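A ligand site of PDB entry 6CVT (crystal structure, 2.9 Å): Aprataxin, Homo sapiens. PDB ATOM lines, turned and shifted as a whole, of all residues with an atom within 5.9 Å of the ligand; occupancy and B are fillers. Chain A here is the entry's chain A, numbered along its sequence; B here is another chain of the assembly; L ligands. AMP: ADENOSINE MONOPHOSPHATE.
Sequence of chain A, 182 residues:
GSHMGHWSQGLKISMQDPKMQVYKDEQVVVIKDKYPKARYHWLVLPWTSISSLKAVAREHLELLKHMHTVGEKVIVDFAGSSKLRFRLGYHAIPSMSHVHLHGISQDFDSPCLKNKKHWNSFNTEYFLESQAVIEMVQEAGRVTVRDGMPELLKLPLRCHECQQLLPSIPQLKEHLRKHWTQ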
ATOM      1  N   TRP A   7     -29.591 -28.242  23.111  1.00  0.00           N
ATOM      2  CA  TRP A   7     -28.240 -28.575  23.564  1.00  0.00           C
ATOM      3  C   TRP A   7     -27.226 -28.256  22.473  1.00  0.00           C
ATOM      4  O   TRP A   7     -26.110 -27.807  22.775  1.00  0.00           O
ATOM      5  CB  TRP A   7     -28.110 -30.048  23.957  1.00  0.00           C
ATOM      6  CG  TRP A   7     -28.325 -31.009  22.823  1.00  0.00           C
ATOM      7  CD1 TRP A   7     -29.492 -31.637  22.496  1.00  0.00           C
ATOM      8  CD2 TRP A   7     -27.349 -31.453  21.862  1.00  0.00           C
ATOM      9  NE1 TRP A   7     -29.299 -32.444  21.395  1.00  0.00           N
ATOM     10  CE2 TRP A   7     -27.997 -32.333  20.982  1.00  0.00           C
ATOM     11  CE3 TRP A   7     -25.994 -31.169  21.662  1.00  0.00           C
ATOM     12  CZ2 TRP A   7     -27.338 -32.943  19.910  1.00  0.00           C
ATOM     13  CZ3 TRP A   7     -25.340 -31.773  20.585  1.00  0.00           C
ATOM     14  CH2 TRP A   7     -26.017 -32.651  19.733  1.00  0.00           C
ATOM     15  N   GLY A  10     -25.765 -24.881  22.718  1.00  0.00           N
ATOM     16  CA  GLY A  10     -25.097 -24.485  23.938  1.00  0.00           C
ATOM     17  C   GLY A  10     -23.902 -23.573  23.716  1.00  0.00           C
ATOM     18  O   GLY A  10     -23.808 -22.497  24.320  1.00  0.00           O
ATOM     19  N   LEU A  11     -23.013 -23.963  22.806  1.00  0.00           N
ATOM     20  CA  LEU A  11     -21.837 -23.127  22.528  1.00  0.00           C
ATOM     21  C   LEU A  11     -22.263 -21.699  22.223  1.00  0.00           C
ATOM     22  O   LEU A  11     -21.809 -20.752  22.872  1.00  0.00           O
ATOM     23  CB  LEU A  11     -21.040 -23.708  21.367  1.00  0.00           C
ATOM     24  CG  LEU A  11     -20.028 -24.813  21.672  1.00  0.00           C
ATOM     25  CD1 LEU A  11     -19.242 -25.139  20.411  1.00  0.00           C
ATOM     26  CD2 LEU A  11     -19.104 -24.347  22.762  1.00  0.00           C
ATOM     27  N   SER A  14     -23.394 -19.950  25.315  1.00  0.00           N
ATOM     28  CA  SER A  14     -22.349 -19.629  26.267  1.00  0.00           C
ATOM     29  C   SER A  14     -21.394 -18.580  25.721  1.00  0.00           C
ATOM     30  O   SER A  14     -20.789 -17.836  26.496  1.00  0.00           O
ATOM     31  CB  SER A  14     -21.607 -20.900  26.654  1.00  0.00           C
ATOM     32  OG  SER A  14     -22.382 -21.649  27.575  1.00  0.00           O
ATOM     33  N   ILE A  31     -13.957 -19.007  25.394  1.00  0.00           N
ATOM     34  CA  ILE A  31     -14.629 -19.471  26.599  1.00  0.00           C
ATOM     35  C   ILE A  31     -13.996 -20.764  27.076  1.00  0.00           C
ATOM     36  O   ILE A  31     -13.376 -21.501  26.302  1.00  0.00           O
ATOM     37  CB  ILE A  31     -16.133 -19.682  26.372  1.00  0.00           C
ATOM     38  CG1 ILE A  31     -16.364 -20.791  25.346  1.00  0.00           C
ATOM     39  CG2 ILE A  31     -16.781 -18.389  25.909  1.00  0.00           C
ATOM     40  CD1 ILE A  31     -17.829 -21.130  25.111  1.00  0.00           C
ATOM     41  N   LYS A  32     -14.143 -21.041  28.372  1.00  0.00           N
ATOM     42  CA  LYS A  32     -13.640 -22.301  28.915  1.00  0.00           C
ATOM     43  C   LYS A  32     -14.552 -23.445  28.498  1.00  0.00           C
ATOM     44  O   LYS A  32     -15.780 -23.323  28.528  1.00  0.00           O
ATOM     45  CB  LYS A  32     -13.560 -22.239  30.447  1.00  0.00           C
ATOM     46  CG  LYS A  32     -12.432 -21.369  30.972  1.00  0.00           C
ATOM     47  CD  LYS A  32     -11.837 -21.934  32.244  1.00  0.00           C
ATOM     48  CE  LYS A  32     -12.684 -21.690  33.463  1.00  0.00           C
ATOM     49  NZ  LYS A  32     -11.894 -22.081  34.678  1.00  0.00           N
ATOM     50  N   ASP A  33     -13.941 -24.570  28.115  1.00  0.00           N
ATOM     51  CA  ASP A  33     -14.702 -25.741  27.710  1.00  0.00           C
ATOM     52  C   ASP A  33     -15.499 -26.271  28.894  1.00  0.00           C
ATOM     53  O   ASP A  33     -14.972 -26.402  30.008  1.00  0.00           O
ATOM     54  CB  ASP A  33     -13.764 -26.826  27.170  1.00  0.00           C
ATOM     55  CG  ASP A  33     -14.502 -27.949  26.458  1.00  0.00           C
ATOM     56  OD1 ASP A  33     -15.157 -28.766  27.136  1.00  0.00           O
ATOM     57  OD2 ASP A  33     -14.427 -28.016  25.213  1.00  0.00           O
ATOM     58  N   LYS A  34     -16.799 -26.488  28.675  1.00  0.00           N
ATOM     59  CA  LYS A  34     -17.673 -26.840  29.781  1.00  0.00           C
ATOM     60  C   LYS A  34     -17.323 -28.204  30.375  1.00  0.00           C
ATOM     61  O   LYS A  34     -17.514 -28.424  31.580  1.00  0.00           O
ATOM     62  CB  LYS A  34     -19.128 -26.821  29.316  1.00  0.00           C
ATOM     63  CG  LYS A  34     -20.113 -26.668  30.460  1.00  0.00           C
ATOM     64  CD  LYS A  34     -21.546 -26.901  30.035  1.00  0.00           C
ATOM     65  CE  LYS A  34     -22.497 -26.677  31.179  1.00  0.00           C
ATOM     66  NZ  LYS A  34     -23.917 -26.826  30.734  1.00  0.00           N
ATOM     67  N   TYR A  35     -16.798 -29.107  29.560  1.00  0.00           N
ATOM     68  CA  TYR A  35     -16.437 -30.462  29.993  1.00  0.00           C
ATOM     69  C   TYR A  35     -14.987 -30.695  29.612  1.00  0.00           C
ATOM     70  O   TYR A  35     -14.679 -31.539  28.758  1.00  0.00           O
ATOM     71  CB  TYR A  35     -17.360 -31.495  29.358  1.00  0.00           C
ATOM     72  CG  TYR A  35     -18.816 -31.144  29.525  1.00  0.00           C
ATOM     73  CD1 TYR A  35     -19.498 -31.513  30.671  1.00  0.00           C
ATOM     74  CD2 TYR A  35     -19.502 -30.443  28.552  1.00  0.00           C
ATOM     75  CE1 TYR A  35     -20.841 -31.197  30.840  1.00  0.00           C
ATOM     76  CE2 TYR A  35     -20.846 -30.112  28.719  1.00  0.00           C
ATOM     77  CZ  TYR A  35     -21.511 -30.495  29.869  1.00  0.00           C
ATOM     78  OH  TYR A  35     -22.844 -30.178  30.048  1.00  0.00           O
ATOM     79  N   PRO A  36     -14.059 -29.955  30.216  1.00  0.00           N
ATOM     80  CA  PRO A  36     -12.691 -29.908  29.703  1.00  0.00           C
ATOM     81  C   PRO A  36     -11.988 -31.249  29.826  1.00  0.00           C
ATOM     82  O   PRO A  36     -12.038 -31.899  30.877  1.00  0.00           O
ATOM     83  CB  PRO A  36     -12.032 -28.838  30.567  1.00  0.00           C
ATOM     84  CG  PRO A  36     -12.785 -28.874  31.816  1.00  0.00           C
ATOM     85  CD  PRO A  36     -14.198 -29.166  31.445  1.00  0.00           C
ATOM     86  N   LYS A  37     -11.299 -31.639  28.756  1.00  0.00           N
ATOM     87  CA  LYS A  37     -10.540 -32.884  28.745  1.00  0.00           C
ATOM     88  C   LYS A  37      -9.122 -32.733  29.302  1.00  0.00           C
ATOM     89  O   LYS A  37      -8.321 -33.669  29.154  1.00  0.00           O
ATOM     90  CB  LYS A  37     -10.477 -33.468  27.324  1.00  0.00           C
ATOM     91  CG  LYS A  37     -11.753 -34.185  26.864  1.00  0.00           C
ATOM     92  CD  LYS A  37     -12.938 -33.276  26.697  1.00  0.00           C
ATOM     93  CE  LYS A  37     -14.226 -34.037  26.770  1.00  0.00           C
ATOM     94  NZ  LYS A  37     -15.367 -33.077  26.714  1.00  0.00           N
ATOM     95  N   HIS A  41      -8.447 -26.051  28.985  1.00  0.00           N
ATOM     96  CA  HIS A  41      -9.143 -26.378  27.747  1.00  0.00           C
ATOM     97  C   HIS A  41     -10.034 -25.189  27.415  1.00  0.00           C
ATOM     98  O   HIS A  41     -10.976 -24.896  28.165  1.00  0.00           O
ATOM     99  CB  HIS A  41      -9.944 -27.675  27.911  1.00  0.00           C
ATOM    100  CG  HIS A  41     -10.433 -28.273  26.630  1.00  0.00           C
ATOM    101  ND1 HIS A  41     -11.225 -29.401  26.591  1.00  0.00           N
ATOM    102  CD2 HIS A  41     -10.271 -27.875  25.339  1.00  0.00           C
ATOM    103  CE1 HIS A  41     -11.518 -29.685  25.329  1.00  0.00           C
ATOM    104  NE2 HIS A  41     -10.959 -28.770  24.549  1.00  0.00           N
ATOM    105  N   LEU A  43     -12.099 -22.900  24.145  1.00  0.00           N
ATOM    106  CA  LEU A  43     -12.665 -22.887  22.800  1.00  0.00           C
ATOM    107  C   LEU A  43     -12.651 -21.460  22.258  1.00  0.00           C
ATOM    108  O   LEU A  43     -13.121 -20.518  22.926  1.00  0.00           O
ATOM    109  CB  LEU A  43     -14.087 -23.441  22.809  1.00  0.00           C
ATOM    110  CG  LEU A  43     -14.198 -24.843  23.395  1.00  0.00           C
ATOM    111  CD1 LEU A  43     -15.623 -25.356  23.384  1.00  0.00           C
ATOM    112  CD2 LEU A  43     -13.322 -25.791  22.625  1.00  0.00           C
ATOM    113  N   HIS A  91     -11.262 -30.393  15.557  1.00  0.00           N
ATOM    114  CA  HIS A  91     -11.766 -31.739  15.341  1.00  0.00           C
ATOM    115  C   HIS A  91     -12.229 -31.896  13.898  1.00  0.00           C
ATOM    116  O   HIS A  91     -12.858 -30.999  13.339  1.00  0.00           O
ATOM    117  CB  HIS A  91     -12.923 -32.035  16.284  1.00  0.00           C
ATOM    118  CG  HIS A  91     -12.496 -32.337  17.680  1.00  0.00           C
ATOM    119  ND1 HIS A  91     -13.395 -32.626  18.686  1.00  0.00           N
ATOM    120  CD2 HIS A  91     -11.264 -32.392  18.249  1.00  0.00           C
ATOM    121  CE1 HIS A  91     -12.734 -32.840  19.814  1.00  0.00           C
ATOM    122  NE2 HIS A  91     -11.439 -32.709  19.577  1.00  0.00           N
ATOM    123  N   ILE A  93     -14.561 -33.959  12.620  1.00  0.00           N
ATOM    124  CA  ILE A  93     -16.022 -33.948  12.692  1.00  0.00           C
ATOM    125  C   ILE A  93     -16.408 -33.289  14.008  1.00  0.00           C
ATOM    126  O   ILE A  93     -16.239 -33.893  15.078  1.00  0.00           O
ATOM    127  CB  ILE A  93     -16.602 -35.369  12.618  1.00  0.00           C
ATOM    128  CG1 ILE A  93     -16.277 -36.044  11.284  1.00  0.00           C
ATOM    129  CG2 ILE A  93     -18.100 -35.307  12.891  1.00  0.00           C
ATOM    130  CD1 ILE A  93     -16.787 -37.485  11.211  1.00  0.00           C
ATOM    131  N   PRO A  94     -16.894 -32.051  13.998  1.00  0.00           N
ATOM    132  CA  PRO A  94     -17.400 -31.469  15.240  1.00  0.00           C
ATOM    133  C   PRO A  94     -18.710 -32.135  15.627  1.00  0.00           C
ATOM    134  O   PRO A  94     -19.454 -32.652  14.781  1.00  0.00           O
ATOM    135  CB  PRO A  94     -17.617 -29.995  14.873  1.00  0.00           C
ATOM    136  CG  PRO A  94     -17.861 -30.011  13.400  1.00  0.00           C
ATOM    137  CD  PRO A  94     -17.025 -31.141  12.845  1.00  0.00           C
ATOM    138  N   SER A  95     -18.975 -32.164  16.929  1.00  0.00           N
ATOM    139  CA  SER A  95     -20.307 -32.557  17.374  1.00  0.00           C
ATOM    140  C   SER A  95     -21.213 -31.336  17.453  1.00  0.00           C
ATOM    141  O   SER A  95     -22.315 -31.349  16.921  1.00  0.00           O
ATOM    142  CB  SER A  95     -20.235 -33.260  18.738  1.00  0.00           C
ATOM    143  OG  SER A  95     -19.265 -34.289  18.740  1.00  0.00           O
ATOM    144  N   MET A  96     -20.733 -30.276  18.107  1.00  0.00           N
ATOM    145  CA  MET A  96     -21.492 -29.043  18.248  1.00  0.00           C
ATOM    146  C   MET A  96     -21.414 -28.203  16.984  1.00  0.00           C
ATOM    147  O   MET A  96     -20.388 -28.180  16.283  1.00  0.00           O
ATOM    148  CB  MET A  96     -20.993 -28.245  19.453  1.00  0.00           C
ATOM    149  CG  MET A  96     -21.068 -28.980  20.785  1.00  0.00           C
ATOM    150  SD  MET A  96     -22.745 -29.197  21.409  1.00  0.00           S
ATOM    151  CE  MET A  96     -22.914 -27.710  22.401  1.00  0.00           C
ATOM    152  N   HIS A  98     -21.052 -25.193  14.329  1.00  0.00           N
ATOM    153  CA  HIS A  98     -20.027 -24.189  14.028  1.00  0.00           C
ATOM    154  C   HIS A  98     -18.620 -24.775  14.128  1.00  0.00           C
ATOM    155  O   HIS A  98     -18.425 -25.850  14.701  1.00  0.00           O
ATOM    156  CB  HIS A  98     -20.166 -22.970  14.942  1.00  0.00           C
ATOM    157  CG  HIS A  98     -21.553 -22.402  14.964  1.00  0.00           C
ATOM    158  ND1 HIS A  98     -22.431 -22.546  13.911  1.00  0.00           N
ATOM    159  CD2 HIS A  98     -22.217 -21.708  15.924  1.00  0.00           C
ATOM    160  CE1 HIS A  98     -23.574 -21.955  14.208  1.00  0.00           C
ATOM    161  NE2 HIS A  98     -23.477 -21.435  15.425  1.00  0.00           N
ATOM    162  N   HIS A 100     -14.932 -24.401  15.746  1.00  0.00           N
ATOM    163  CA  HIS A 100     -14.359 -23.843  16.957  1.00  0.00           C
ATOM    164  C   HIS A 100     -12.961 -24.400  17.174  1.00  0.00           C
ATOM    165  O   HIS A 100     -12.726 -25.598  16.970  1.00  0.00           O
ATOM    166  CB  HIS A 100     -15.255 -24.117  18.178  1.00  0.00           C
ATOM    167  CG  HIS A 100     -16.068 -25.364  18.070  1.00  0.00           C
ATOM    168  ND1 HIS A 100     -17.198 -25.453  17.273  1.00  0.00           N
ATOM    169  CD2 HIS A 100     -15.953 -26.571  18.685  1.00  0.00           C
ATOM    170  CE1 HIS A 100     -17.714 -26.661  17.376  1.00  0.00           C
ATOM    171  NE2 HIS A 100     -16.982 -27.357  18.225  1.00  0.00           N
ATOM    172  N   HIS A 102      -9.784 -25.587  19.368  1.00  0.00           N
ATOM    173  CA  HIS A 102      -9.449 -26.166  20.661  1.00  0.00           C
ATOM    174  C   HIS A 102      -8.042 -25.745  21.046  1.00  0.00           C
ATOM    175  O   HIS A 102      -7.094 -25.954  20.283  1.00  0.00           O
ATOM    176  CB  HIS A 102      -9.540 -27.693  20.649  1.00  0.00           C
ATOM    177  CG  HIS A 102     -10.932 -28.224  20.587  1.00  0.00           C
ATOM    178  ND1 HIS A 102     -11.614 -28.659  21.708  1.00  0.00           N
ATOM    179  CD2 HIS A 102     -11.774 -28.416  19.532  1.00  0.00           C
ATOM    180  CE1 HIS A 102     -12.810 -29.091  21.353  1.00  0.00           C
ATOM    181  NE2 HIS A 102     -12.939 -28.959  20.044  1.00  0.00           N
ATOM    182  N   LYS A 117     -13.417 -42.337  22.717  1.00  0.00           N
ATOM    183  CA  LYS A 117     -13.743 -41.278  21.755  1.00  0.00           C
ATOM    184  C   LYS A 117     -13.015 -39.985  22.103  1.00  0.00           C
ATOM    185  O   LYS A 117     -12.410 -39.367  21.232  1.00  0.00           O
ATOM    186  CB  LYS A 117     -15.257 -41.051  21.701  1.00  0.00           C
ATOM    187  CG  LYS A 117     -15.741 -40.276  20.471  1.00  0.00           C
ATOM    188  CD  LYS A 117     -16.052 -38.826  20.808  1.00  0.00           C
ATOM    189  CE  LYS A 117     -15.044 -37.831  20.205  1.00  0.00           C
ATOM    190  NZ  LYS A 117     -14.916 -36.557  21.000  1.00  0.00           N
ATOM    191  N   PHE A 122      -8.521 -36.290  20.552  1.00  0.00           N
ATOM    192  CA  PHE A 122      -7.429 -35.340  20.736  1.00  0.00           C
ATOM    193  C   PHE A 122      -6.051 -35.908  20.434  1.00  0.00           C
ATOM    194  O   PHE A 122      -5.076 -35.140  20.471  1.00  0.00           O
ATOM    195  CB  PHE A 122      -7.448 -34.768  22.174  1.00  0.00           C
ATOM    196  CG  PHE A 122      -8.565 -33.808  22.384  1.00  0.00           C
ATOM    197  CD1 PHE A 122      -8.433 -32.477  21.983  1.00  0.00           C
ATOM    198  CD2 PHE A 122      -9.773 -34.221  22.928  1.00  0.00           C
ATOM    199  CE1 PHE A 122      -9.483 -31.591  22.152  1.00  0.00           C
ATOM    200  CE2 PHE A 122     -10.814 -33.334  23.108  1.00  0.00           C
ATOM    201  CZ  PHE A 122     -10.666 -32.022  22.723  1.00  0.00           C
ATOM    202  OP3   G B   1     -17.818 -36.234  20.259  1.00  0.00           O
ATOM    203  P     G B   1     -18.702 -36.356  21.596  1.00  0.00           P
ATOM    204  OP1   G B   1     -18.324 -37.556  22.378  1.00  0.00           O
ATOM    205  OP2   G B   1     -20.124 -36.240  21.200  1.00  0.00           O
ATOM    206  O5'   G B   1     -18.326 -35.106  22.516  1.00  0.00           O
ATOM    207  C5'   G B   1     -18.422 -33.777  22.011  1.00  0.00           C
ATOM    208  C4'   G B   1     -19.336 -32.942  22.879  1.00  0.00           C
ATOM    209  O4'   G B   1     -20.535 -32.639  22.126  1.00  0.00           O
ATOM    210  C3'   G B   1     -19.845 -33.666  24.111  1.00  0.00           C
ATOM    211  O3'   G B   1     -18.936 -33.605  25.200  1.00  0.00           O
ATOM    212  C2'   G B   1     -21.200 -32.995  24.372  1.00  0.00           C
ATOM    213  O2'   G B   1     -21.041 -31.757  25.059  1.00  0.00           O
ATOM    214  C1'   G B   1     -21.667 -32.674  22.963  1.00  0.00           C
ATOM    215  N9    G B   1     -22.664 -33.623  22.404  1.00  0.00           N
ATOM    216  C8    G B   1     -22.572 -34.365  21.238  1.00  0.00           C
ATOM    217  N7    G B   1     -23.648 -35.059  20.966  1.00  0.00           N
ATOM    218  C5    G B   1     -24.517 -34.744  22.001  1.00  0.00           C
ATOM    219  C6    G B   1     -25.841 -35.185  22.273  1.00  0.00           C
ATOM    220  O6    G B   1     -26.539 -35.976  21.635  1.00  0.00           O
ATOM    221  N1    G B   1     -26.344 -34.609  23.433  1.00  0.00           N
ATOM    222  C2    G B   1     -25.678 -33.727  24.245  1.00  0.00           C
ATOM    223  N2    G B   1     -26.321 -33.263  25.343  1.00  0.00           N
ATOM    224  N3    G B   1     -24.453 -33.305  24.003  1.00  0.00           N
ATOM    225  C4    G B   1     -23.934 -33.849  22.885  1.00  0.00           C
ATOM    226  P    DT B   2     -18.774 -34.885  26.153  1.00  0.00           P
ATOM    227  OP1  DT B   2     -17.641 -34.707  27.090  1.00  0.00           O
ATOM    228  OP2  DT B   2     -18.784 -36.048  25.242  1.00  0.00           O
ATOM    229  O5'  DT B   2     -20.102 -34.854  27.029  1.00  0.00           O
ATOM    230  C5'  DT B   2     -20.436 -33.693  27.763  1.00  0.00           C
ATOM    231  C4'  DT B   2     -21.743 -33.902  28.477  1.00  0.00           C
ATOM    232  O4'  DT B   2     -22.762 -34.146  27.503  1.00  0.00           O
ATOM    233  C3'  DT B   2     -21.732 -35.113  29.415  1.00  0.00           C
ATOM    234  O3'  DT B   2     -21.991 -34.729  30.737  1.00  0.00           O
ATOM    235  C2'  DT B   2     -22.818 -36.039  28.893  1.00  0.00           C
ATOM    236  C1'  DT B   2     -23.592 -35.205  27.906  1.00  0.00           C
ATOM    237  N1   DT B   2     -23.953 -35.952  26.709  1.00  0.00           N
ATOM    238  C2   DT B   2     -25.228 -36.438  26.577  1.00  0.00           C
ATOM    239  O2   DT B   2     -26.089 -36.265  27.417  1.00  0.00           O
ATOM    240  N3   DT B   2     -25.456 -37.138  25.425  1.00  0.00           N
ATOM    241  C4   DT B   2     -24.552 -37.401  24.421  1.00  0.00           C
ATOM    242  O4   DT B   2     -24.855 -38.034  23.417  1.00  0.00           O
ATOM    243  C5   DT B   2     -23.227 -36.860  24.629  1.00  0.00           C
ATOM    244  C7   DT B   2     -22.155 -37.068  23.592  1.00  0.00           C
ATOM    245  C6   DT B   2     -22.999 -36.183  25.753  1.00  0.00           C
HETATM  246  P   AMP L   1     -16.135 -30.161  18.954  1.00  0.00           P
HETATM  247  O1P AMP L   1     -15.662 -31.518  19.445  1.00  0.00           O
HETATM  248  O2P AMP L   1     -15.228 -29.323  18.075  1.00  0.00           O
HETATM  249  O3P AMP L   1     -17.551 -30.431  18.236  1.00  0.00           O
HETATM  250  O5' AMP L   1     -16.415 -29.223  20.201  1.00  0.00           O
HETATM  251  C5' AMP L   1     -17.291 -29.623  21.253  1.00  0.00           C
HETATM  252  C4' AMP L   1     -16.735 -29.170  22.569  1.00  0.00           C
HETATM  253  O4' AMP L   1     -17.601 -28.181  23.146  1.00  0.00           O
HETATM  254  C3' AMP L   1     -16.586 -30.295  23.612  1.00  0.00           C
HETATM  255  O3' AMP L   1     -15.236 -30.388  24.047  1.00  0.00           O
HETATM  256  C2' AMP L   1     -17.492 -29.856  24.773  1.00  0.00           C
HETATM  257  O2' AMP L   1     -16.948 -30.131  26.043  1.00  0.00           O
HETATM  258  C1' AMP L   1     -17.644 -28.357  24.541  1.00  0.00           C
HETATM  259  N9  AMP L   1     -18.894 -27.780  25.044  1.00  0.00           N
HETATM  260  C8  AMP L   1     -20.133 -28.360  24.983  1.00  0.00           C
HETATM  261  N7  AMP L   1     -21.096 -27.595  25.506  1.00  0.00           N
HETATM  262  C5  AMP L   1     -20.431 -26.438  25.928  1.00  0.00           C
HETATM  263  C6  AMP L   1     -20.880 -25.251  26.544  1.00  0.00           C
HETATM  264  N6  AMP L   1     -22.168 -25.014  26.874  1.00  0.00           N
HETATM  265  N1  AMP L   1     -19.946 -24.309  26.826  1.00  0.00           N
HETATM  266  C2  AMP L   1     -18.669 -24.539  26.497  1.00  0.00           C
HETATM  267  N3  AMP L   1     -18.140 -25.609  25.911  1.00  0.00           N
HETATM  268  C4  AMP L   1     -19.076 -26.558  25.642  1.00  0.00           C
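N of Lys 34 sits at hydrogen-bond distance from N3 of the ligand, 3.2 Å away.
A ring nitrogen (ND1) of His 91 lies within hydrogen-bond range of an oxygen (O1P) of the ligand (2.6 Å).
NZ of Lys 37 lies within hydrogen-bond range of O2' of the ligand.
An oxygen (O2P) of the ligand is in hydrogen-bond range of a ring nitrogen (NE2) of His 102, 3.0 Å away.
O3P of the ligand sits at hydrogen-bond distance from N of Met 96 (3.2 Å).
An oxygen (O2P) of the ligand sits at hydrogen-bond distance from a ring nitrogen (NE2) of His 100 (2.6 Å).
An oxygen (O2') of the ligand sits at hydrogen-bond distance from the side-chain carboxylate (OD1) of Asp 33, 2.5 Å away.
The side-chain hydroxyl (OG) of Ser 14 sits at hydrogen-bond distance from a nitrogen (N6) of the ligand (3.4 Å).
An oxygen (O3P) of the ligand lies within hydrogen-bond range of the backbone NH of Ser 95, 2.6 Å away.
The backbone NH (N) of Lys 37 lies within hydrogen-bond range of a ring nitrogen (ND1) of His 41 (3.1 Å).
The backbone NH (N) of Leu 43 sits at hydrogen-bond distance from the backbone carbonyl oxygen (O) of Ile 31.
OG of Ser 95 sits at hydrogen-bond distance from OP3 of G 1 of chain B (2.9 Å).
OP3 of G 1 of chain B lies within salt-bridge range of the side-chain amino group (NZ) of Lys 117 (3.0 Å).
NE2 of His 41 lies within hydrogen-bond range of ND1 of His 102, at 2.9 Å.
The backbone NH (N) of Tyr 35 sits at hydrogen-bond distance from the side-chain carboxylate (OD1) of Asp 33 (2.9 Å).
ND1 of His 100 sits at hydrogen-bond distance from O of His 98, 2.9 Å away.
NZ of Lys 37 is in hydrogen-bond range of O of Tyr 35 (2.6 Å).
Residues that only touch the ligand: Gly 10, Leu 11, Ile 31, Lys 32, Tyr 35, His 41, Leu 43, Pro 94 and G 1 of chain B.
Hydrophobic or aromatic side chains that line the ligand: Leu 11, Ile 31, Tyr 35, His 41, Leu 43, His 91, Pro 94, Met 96, His 100 and His 102.
Within 4 Å of the ligand: Gly 10, Leu 11, Ser 14, Ile 31, Lys 32, Asp 33, Lys 34, Tyr 35, Lys 37, His 41, Leu 43, His 91, Pro 94, Ser 95, Met 96, His 100, His 102 and G 1 of chain B.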
